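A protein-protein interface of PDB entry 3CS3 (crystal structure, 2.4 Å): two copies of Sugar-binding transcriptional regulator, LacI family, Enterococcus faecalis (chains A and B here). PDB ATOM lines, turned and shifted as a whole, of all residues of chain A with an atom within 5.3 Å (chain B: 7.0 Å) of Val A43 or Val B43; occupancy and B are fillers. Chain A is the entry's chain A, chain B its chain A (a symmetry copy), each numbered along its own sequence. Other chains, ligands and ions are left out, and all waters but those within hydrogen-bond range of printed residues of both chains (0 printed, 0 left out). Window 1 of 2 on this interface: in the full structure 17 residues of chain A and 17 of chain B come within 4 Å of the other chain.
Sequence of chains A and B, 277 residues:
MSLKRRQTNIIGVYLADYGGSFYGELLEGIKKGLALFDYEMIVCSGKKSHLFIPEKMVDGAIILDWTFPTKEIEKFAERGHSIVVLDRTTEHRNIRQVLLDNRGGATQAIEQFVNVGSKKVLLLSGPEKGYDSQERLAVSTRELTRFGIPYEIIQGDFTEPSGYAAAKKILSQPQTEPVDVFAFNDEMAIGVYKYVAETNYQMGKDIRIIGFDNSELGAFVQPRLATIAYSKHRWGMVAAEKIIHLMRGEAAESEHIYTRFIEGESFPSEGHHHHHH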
ATOM      1  N   VAL A  13     -17.393 -23.850  23.311  1.00  0.00           N
ATOM      2  CA  VAL A  13     -16.239 -22.973  23.197  1.00  0.00           C
ATOM      3  C   VAL A  13     -16.539 -21.681  23.950  1.00  0.00           C
ATOM      4  O   VAL A  13     -17.461 -20.951  23.603  1.00  0.00           O
ATOM      5  CB  VAL A  13     -15.860 -22.710  21.726  1.00  0.00           C
ATOM      6  CG1 VAL A  13     -14.681 -21.756  21.634  1.00  0.00           C
ATOM      7  CG2 VAL A  13     -15.532 -24.027  21.015  1.00  0.00           C
ATOM      8  N   LEU A  15     -15.549 -18.105  24.966  1.00  0.00           N
ATOM      9  CA  LEU A  15     -14.750 -16.944  24.582  1.00  0.00           C
ATOM     10  C   LEU A  15     -15.082 -15.753  25.465  1.00  0.00           C
ATOM     11  O   LEU A  15     -16.122 -15.730  26.115  1.00  0.00           O
ATOM     12  CB  LEU A  15     -14.955 -16.599  23.105  1.00  0.00           C
ATOM     13  CG  LEU A  15     -14.625 -17.691  22.076  1.00  0.00           C
ATOM     14  CD1 LEU A  15     -14.836 -17.140  20.687  1.00  0.00           C
ATOM     15  CD2 LEU A  15     -13.198 -18.254  22.224  1.00  0.00           C
ATOM     16  N   LEU A  27     -11.961 -19.793  15.480  1.00  0.00           N
ATOM     17  CA  LEU A  27     -13.201 -20.565  15.383  1.00  0.00           C
ATOM     18  C   LEU A  27     -13.304 -21.437  14.128  1.00  0.00           C
ATOM     19  O   LEU A  27     -13.837 -22.544  14.199  1.00  0.00           O
ATOM     20  CB  LEU A  27     -14.416 -19.635  15.480  1.00  0.00           C
ATOM     21  CG  LEU A  27     -15.102 -19.385  16.835  1.00  0.00           C
ATOM     22  CD1 LEU A  27     -14.297 -19.861  18.044  1.00  0.00           C
ATOM     23  CD2 LEU A  27     -15.443 -17.913  16.978  1.00  0.00           C
ATOM     24  N   MET A  41     -19.559 -27.442  17.235  1.00  0.00           N
ATOM     25  CA  MET A  41     -19.203 -26.517  18.283  1.00  0.00           C
ATOM     26  C   MET A  41     -20.297 -25.491  18.552  1.00  0.00           C
ATOM     27  O   MET A  41     -21.006 -25.070  17.641  1.00  0.00           O
ATOM     28  CB  MET A  41     -17.835 -25.893  17.965  1.00  0.00           C
ATOM     29  CG  MET A  41     -17.766 -24.392  17.899  1.00  0.00           C
ATOM     30  SD  MET A  41     -16.418 -23.924  16.813  1.00  0.00           S
ATOM     31  CE  MET A  41     -17.141 -22.485  16.016  1.00  0.00           C
ATOM     32  N   ILE A  42     -20.479 -25.153  19.823  1.00  0.00           N
ATOM     33  CA  ILE A  42     -21.238 -23.962  20.173  1.00  0.00           C
ATOM     34  C   ILE A  42     -20.332 -22.979  20.899  1.00  0.00           C
ATOM     35  O   ILE A  42     -19.440 -23.376  21.654  1.00  0.00           O
ATOM     36  CB  ILE A  42     -22.528 -24.252  20.982  1.00  0.00           C
ATOM     37  CG1 ILE A  42     -22.229 -25.071  22.235  1.00  0.00           C
ATOM     38  CG2 ILE A  42     -23.545 -24.952  20.095  1.00  0.00           C
ATOM     39  CD1 ILE A  42     -22.722 -24.420  23.511  1.00  0.00           C
ATOM     40  N   VAL A  43     -20.547 -21.696  20.638  1.00  0.00           N
ATOM     41  CA  VAL A  43     -19.717 -20.654  21.211  1.00  0.00           C
ATOM     42  C   VAL A  43     -20.540 -19.870  22.221  1.00  0.00           C
ATOM     43  O   VAL A  43     -21.656 -19.456  21.921  1.00  0.00           O
ATOM     44  CB  VAL A  43     -19.147 -19.723  20.119  1.00  0.00           C
ATOM     45  CG1 VAL A  43     -18.245 -18.655  20.725  1.00  0.00           C
ATOM     46  CG2 VAL A  43     -18.382 -20.524  19.081  1.00  0.00           C
ATOM     47  N   CYS A  44     -19.989 -19.689  23.419  1.00  0.00           N
ATOM     48  CA  CYS A  44     -20.641 -18.913  24.463  1.00  0.00           C
ATOM     49  C   CYS A  44     -19.729 -17.821  24.988  1.00  0.00           C
ATOM     50  O   CYS A  44     -18.529 -18.024  25.145  1.00  0.00           O
ATOM     51  CB  CYS A  44     -21.094 -19.814  25.606  1.00  0.00           C
ATOM     52  SG  CYS A  44     -22.319 -21.018  25.084  1.00  0.00           S
ATOM     53  N   SER A  45     -20.309 -16.660  25.259  1.00  0.00           N
ATOM     54  CA  SER A  45     -19.538 -15.520  25.721  1.00  0.00           C
ATOM     55  C   SER A  45     -20.328 -14.668  26.707  1.00  0.00           C
ATOM     56  O   SER A  45     -21.548 -14.595  26.633  1.00  0.00           O
ATOM     57  CB  SER A  45     -19.101 -14.676  24.529  1.00  0.00           C
ATOM     58  OG  SER A  45     -18.022 -13.853  24.903  1.00  0.00           O
ATOM     59  N   GLY A  46     -19.623 -14.022  27.627  1.00  0.00           N
ATOM     60  CA  GLY A  46     -20.259 -13.186  28.638  1.00  0.00           C
ATOM     61  C   GLY A  46     -19.683 -13.421  30.019  1.00  0.00           C
ATOM     62  O   GLY A  46     -19.053 -14.451  30.268  1.00  0.00           O
ATOM     63  N   ILE B  11     -30.108 -11.600  29.701  1.00  0.00           N
ATOM     64  CA  ILE B  11     -30.688 -11.764  28.373  1.00  0.00           C
ATOM     65  C   ILE B  11     -29.758 -12.641  27.539  1.00  0.00           C
ATOM     66  O   ILE B  11     -28.555 -12.397  27.486  1.00  0.00           O
ATOM     67  CB  ILE B  11     -30.939 -10.387  27.677  1.00  0.00           C
ATOM     68  CG1 ILE B  11     -31.866  -9.498  28.527  1.00  0.00           C
ATOM     69  CG2 ILE B  11     -31.492 -10.564  26.256  1.00  0.00           C
ATOM     70  CD1 ILE B  11     -33.257 -10.090  28.811  1.00  0.00           C
ATOM     71  N   GLY B  12     -30.314 -13.684  26.930  1.00  0.00           N
ATOM     72  CA  GLY B  12     -29.572 -14.508  25.976  1.00  0.00           C
ATOM     73  C   GLY B  12     -29.578 -13.874  24.596  1.00  0.00           C
ATOM     74  O   GLY B  12     -30.629 -13.525  24.071  1.00  0.00           O
ATOM     75  N   VAL B  13     -28.400 -13.704  24.010  1.00  0.00           N
ATOM     76  CA  VAL B  13     -28.296 -13.117  22.684  1.00  0.00           C
ATOM     77  C   VAL B  13     -27.809 -14.191  21.717  1.00  0.00           C
ATOM     78  O   VAL B  13     -26.709 -14.715  21.862  1.00  0.00           O
ATOM     79  CB  VAL B  13     -27.382 -11.874  22.676  1.00  0.00           C
ATOM     80  CG1 VAL B  13     -27.254 -11.307  21.273  1.00  0.00           C
ATOM     81  CG2 VAL B  13     -27.923 -10.806  23.631  1.00  0.00           C
ATOM     82  N   TYR B  14     -28.650 -14.531  20.747  1.00  0.00           N
ATOM     83  CA  TYR B  14     -28.357 -15.627  19.831  1.00  0.00           C
ATOM     84  C   TYR B  14     -27.919 -15.107  18.470  1.00  0.00           C
ATOM     85  O   TYR B  14     -28.723 -14.577  17.701  1.00  0.00           O
ATOM     86  CB  TYR B  14     -29.547 -16.595  19.741  1.00  0.00           C
ATOM     87  CG  TYR B  14     -29.766 -17.338  21.039  1.00  0.00           C
ATOM     88  CD1 TYR B  14     -29.132 -18.555  21.278  1.00  0.00           C
ATOM     89  CD2 TYR B  14     -30.571 -16.800  22.050  1.00  0.00           C
ATOM     90  CE1 TYR B  14     -29.306 -19.231  22.473  1.00  0.00           C
ATOM     91  CE2 TYR B  14     -30.749 -17.466  23.251  1.00  0.00           C
ATOM     92  CZ  TYR B  14     -30.116 -18.684  23.451  1.00  0.00           C
ATOM     93  OH  TYR B  14     -30.283 -19.358  24.637  1.00  0.00           O
ATOM     94  N   LEU B  15     -26.621 -15.232  18.210  1.00  0.00           N
ATOM     95  CA  LEU B  15     -26.006 -14.748  16.976  1.00  0.00           C
ATOM     96  C   LEU B  15     -25.650 -15.911  16.067  1.00  0.00           C
ATOM     97  O   LEU B  15     -25.569 -17.051  16.514  1.00  0.00           O
ATOM     98  CB  LEU B  15     -24.771 -13.895  17.276  1.00  0.00           C
ATOM     99  CG  LEU B  15     -24.972 -12.652  18.157  1.00  0.00           C
ATOM    100  CD1 LEU B  15     -23.659 -11.920  18.284  1.00  0.00           C
ATOM    101  CD2 LEU B  15     -26.071 -11.707  17.633  1.00  0.00           C
ATOM    102  N   ASP B  17     -22.884 -15.857  13.913  1.00  0.00           N
ATOM    103  CA  ASP B  17     -21.441 -15.793  13.618  1.00  0.00           C
ATOM    104  C   ASP B  17     -21.037 -15.798  12.136  1.00  0.00           C
ATOM    105  O   ASP B  17     -20.092 -16.481  11.731  1.00  0.00           O
ATOM    106  CB  ASP B  17     -20.600 -16.773  14.456  1.00  0.00           C
ATOM    107  CG  ASP B  17     -19.922 -16.096  15.644  1.00  0.00           C
ATOM    108  OD1 ASP B  17     -18.700 -16.290  15.821  1.00  0.00           O
ATOM    109  OD2 ASP B  17     -20.603 -15.361  16.395  1.00  0.00           O
ATOM    110  N   TYR B  23     -21.092  -7.156  14.735  1.00  0.00           N
ATOM    111  CA  TYR B  23     -21.480  -7.723  16.038  1.00  0.00           C
ATOM    112  C   TYR B  23     -20.934  -6.953  17.224  1.00  0.00           C
ATOM    113  O   TYR B  23     -21.668  -6.689  18.168  1.00  0.00           O
ATOM    114  CB  TYR B  23     -21.080  -9.196  16.180  1.00  0.00           C
ATOM    115  CG  TYR B  23     -21.987 -10.172  15.472  1.00  0.00           C
ATOM    116  CD1 TYR B  23     -23.293  -9.822  15.118  1.00  0.00           C
ATOM    117  CD2 TYR B  23     -21.547 -11.459  15.169  1.00  0.00           C
ATOM    118  CE1 TYR B  23     -24.127 -10.721  14.463  1.00  0.00           C
ATOM    119  CE2 TYR B  23     -22.375 -12.364  14.512  1.00  0.00           C
ATOM    120  CZ  TYR B  23     -23.664 -11.990  14.167  1.00  0.00           C
ATOM    121  OH  TYR B  23     -24.486 -12.887  13.519  1.00  0.00           O
ATOM    122  N   LEU B  27     -23.398  -5.617  19.903  1.00  0.00           N
ATOM    123  CA  LEU B  27     -23.264  -6.133  21.267  1.00  0.00           C
ATOM    124  C   LEU B  27     -22.988  -5.060  22.323  1.00  0.00           C
ATOM    125  O   LEU B  27     -23.493  -5.161  23.441  1.00  0.00           O
ATOM    126  CB  LEU B  27     -22.183  -7.219  21.321  1.00  0.00           C
ATOM    127  CG  LEU B  27     -22.558  -8.704  21.183  1.00  0.00           C
ATOM    128  CD1 LEU B  27     -23.981  -8.948  20.680  1.00  0.00           C
ATOM    129  CD2 LEU B  27     -21.558  -9.409  20.284  1.00  0.00           C
ATOM    130  N   MET B  41     -25.903  -9.727  29.708  1.00  0.00           N
ATOM    131  CA  MET B  41     -26.132 -10.505  28.515  1.00  0.00           C
ATOM    132  C   MET B  41     -25.152 -11.663  28.376  1.00  0.00           C
ATOM    133  O   MET B  41     -23.994 -11.560  28.772  1.00  0.00           O
ATOM    134  CB  MET B  41     -26.159  -9.567  27.298  1.00  0.00           C
ATOM    135  CG  MET B  41     -25.194  -9.865  26.182  1.00  0.00           C
ATOM    136  SD  MET B  41     -24.830  -8.341  25.310  1.00  0.00           S
ATOM    137  CE  MET B  41     -23.091  -8.597  24.943  1.00  0.00           C
ATOM    138  N   ILE B  42     -25.648 -12.790  27.880  1.00  0.00           N
ATOM    139  CA  ILE B  42     -24.766 -13.837  27.389  1.00  0.00           C
ATOM    140  C   ILE B  42     -25.006 -14.046  25.901  1.00  0.00           C
ATOM    141  O   ILE B  42     -26.135 -13.924  25.417  1.00  0.00           O
ATOM    142  CB  ILE B  42     -24.869 -15.169  28.175  1.00  0.00           C
ATOM    143  CG1 ILE B  42     -26.308 -15.676  28.226  1.00  0.00           C
ATOM    144  CG2 ILE B  42     -24.299 -14.988  29.572  1.00  0.00           C
ATOM    145  CD1 ILE B  42     -26.468 -17.086  27.696  1.00  0.00           C
ATOM    146  N   VAL B  43     -23.930 -14.327  25.177  1.00  0.00           N
ATOM    147  CA  VAL B  43     -24.003 -14.487  23.737  1.00  0.00           C
ATOM    148  C   VAL B  43     -23.762 -15.948  23.394  1.00  0.00           C
ATOM    149  O   VAL B  43     -22.804 -16.548  23.876  1.00  0.00           O
ATOM    150  CB  VAL B  43     -22.987 -13.574  23.018  1.00  0.00           C
ATOM    151  CG1 VAL B  43     -23.097 -13.719  21.505  1.00  0.00           C
ATOM    152  CG2 VAL B  43     -23.195 -12.124  23.418  1.00  0.00           C
ATOM    153  N   CYS B  44     -24.645 -16.516  22.576  1.00  0.00           N
ATOM    154  CA  CYS B  44     -24.508 -17.892  22.122  1.00  0.00           C
ATOM    155  C   CYS B  44     -24.557 -17.978  20.609  1.00  0.00           C
ATOM    156  O   CYS B  44     -25.327 -17.277  19.962  1.00  0.00           O
ATOM    157  CB  CYS B  44     -25.589 -18.776  22.734  1.00  0.00           C
ATOM    158  SG  CYS B  44     -25.471 -18.861  24.524  1.00  0.00           S
ATOM    159  N   SER B  45     -23.724 -18.846  20.049  1.00  0.00           N
ATOM    160  CA  SER B  45     -23.639 -18.989  18.607  1.00  0.00           C
ATOM    161  C   SER B  45     -23.355 -20.430  18.200  1.00  0.00           C
ATOM    162  O   SER B  45     -22.708 -21.170  18.930  1.00  0.00           O
ATOM    163  CB  SER B  45     -22.556 -18.064  18.061  1.00  0.00           C
ATOM    164  OG  SER B  45     -22.757 -17.866  16.682  1.00  0.00           O
ATOM    165  N   GLY B  46     -23.839 -20.819  17.028  1.00  0.00           N
ATOM    166  CA  GLY B  46     -23.651 -22.176  16.529  1.00  0.00           C
ATOM    167  C   GLY B  46     -24.924 -22.753  15.946  1.00  0.00           C
ATOM    168  O   GLY B  46     -26.020 -22.266  16.230  1.00  0.00           O
ATOM    169  N   SER B  49     -27.144 -24.237  18.768  1.00  0.00           N
ATOM    170  CA  SER B  49     -27.271 -23.351  19.937  1.00  0.00           C
ATOM    171  C   SER B  49     -28.709 -23.175  20.440  1.00  0.00           C
ATOM    172  O   SER B  49     -28.925 -22.874  21.618  1.00  0.00           O
ATOM    173  CB  SER B  49     -26.649 -21.983  19.649  1.00  0.00           C
ATOM    174  OG  SER B  49     -27.411 -21.269  18.690  1.00  0.00           O
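O of Ser B45 is in hydrogen-bond range of N of Val A43. N of Val B43 lies within hydrogen-bond range of O of Ser A45 (2.8 Å).
The backbone NH of Val A13 lies within hydrogen-bond range of the backbone carbonyl oxygen of Ile A42. O of Ile B42 is in hydrogen-bond range of N of Val B13, 2.7 Å away. O of Val B13 lies within hydrogen-bond range of N of Cys B44 (2.8 Å). The backbone NH of Leu B15 lies within hydrogen-bond range of the backbone carbonyl oxygen of Cys B44, 3.0 Å away. The side-chain hydroxyl (OH) of Tyr B23 lies within hydrogen-bond range of the backbone NH (N) of Asp B17 (3.4 Å). The backbone carbonyl oxygen (O) of Gly B46 sits at hydrogen-bond distance from the side-chain hydroxyl (OG) of Ser B49.
CD2 of Leu A27 touches OD1 of Asp B17 (3.8 Å). Ser B45 touches Ile A42. Ile A42 touches Ser B49. Val A43 touches Val B43. Val A43 touches Cys B44 (O to CA, 3.3 Å). Cys A44 touches Val B43 (CA to O, 3.3 Å). Cys B44 touches Cys A44. CA of Ile B42 touches O of Ser A45 (3.4 Å).
Of chain B, only Val B43, Cys B44 and Ser B45 come within 4 Å of Val A43. Of the printed residues of chain B, Cys A44 touches Val B43 (3.3 Å) and Cys B44 (3.9 Å). Printed residues of chain A within 4 Å of Asp B17: Leu A27 (3.8 Å). Gly B46 touches none of the printed residues of chain A. The nearest residue of chain B that does not touch Val A43 is Gly B46 (5.0 Å). The nearest residue of chain A that does not touch Val B43 is Gly A46 (5.0 Å). The nearest printed residue of chain B that does not touch Leu A27 is Ser B45 (7.2 Å).
Hydrophobic or aromatic side chains of chain B within 4 Å of the printed part of chain A: Ile B42. Of the 9 printed residues of chain A, 5 touch a printed residue of chain B. Printed residues of chain A that touch a printed residue of chain B: Leu A27, Ile A42, Val A43, Cys A44 and Ser A45. Among the printed residues, no Asp or Glu carboxylate lies within 4 Å of a Lys or Arg side-chain nitrogen of the other chain.
Ile A42 touches Ser B45, and with the chains exchanged Ser A45 touches Ile B42. Val A43 touches its own counterpart, Val B43. Val A43 touches Ser B45, and with the chains exchanged Ser A45 touches Val B43. Cys A44 touches its own counterpart, Cys B44. 9 positions are printed for both chains.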
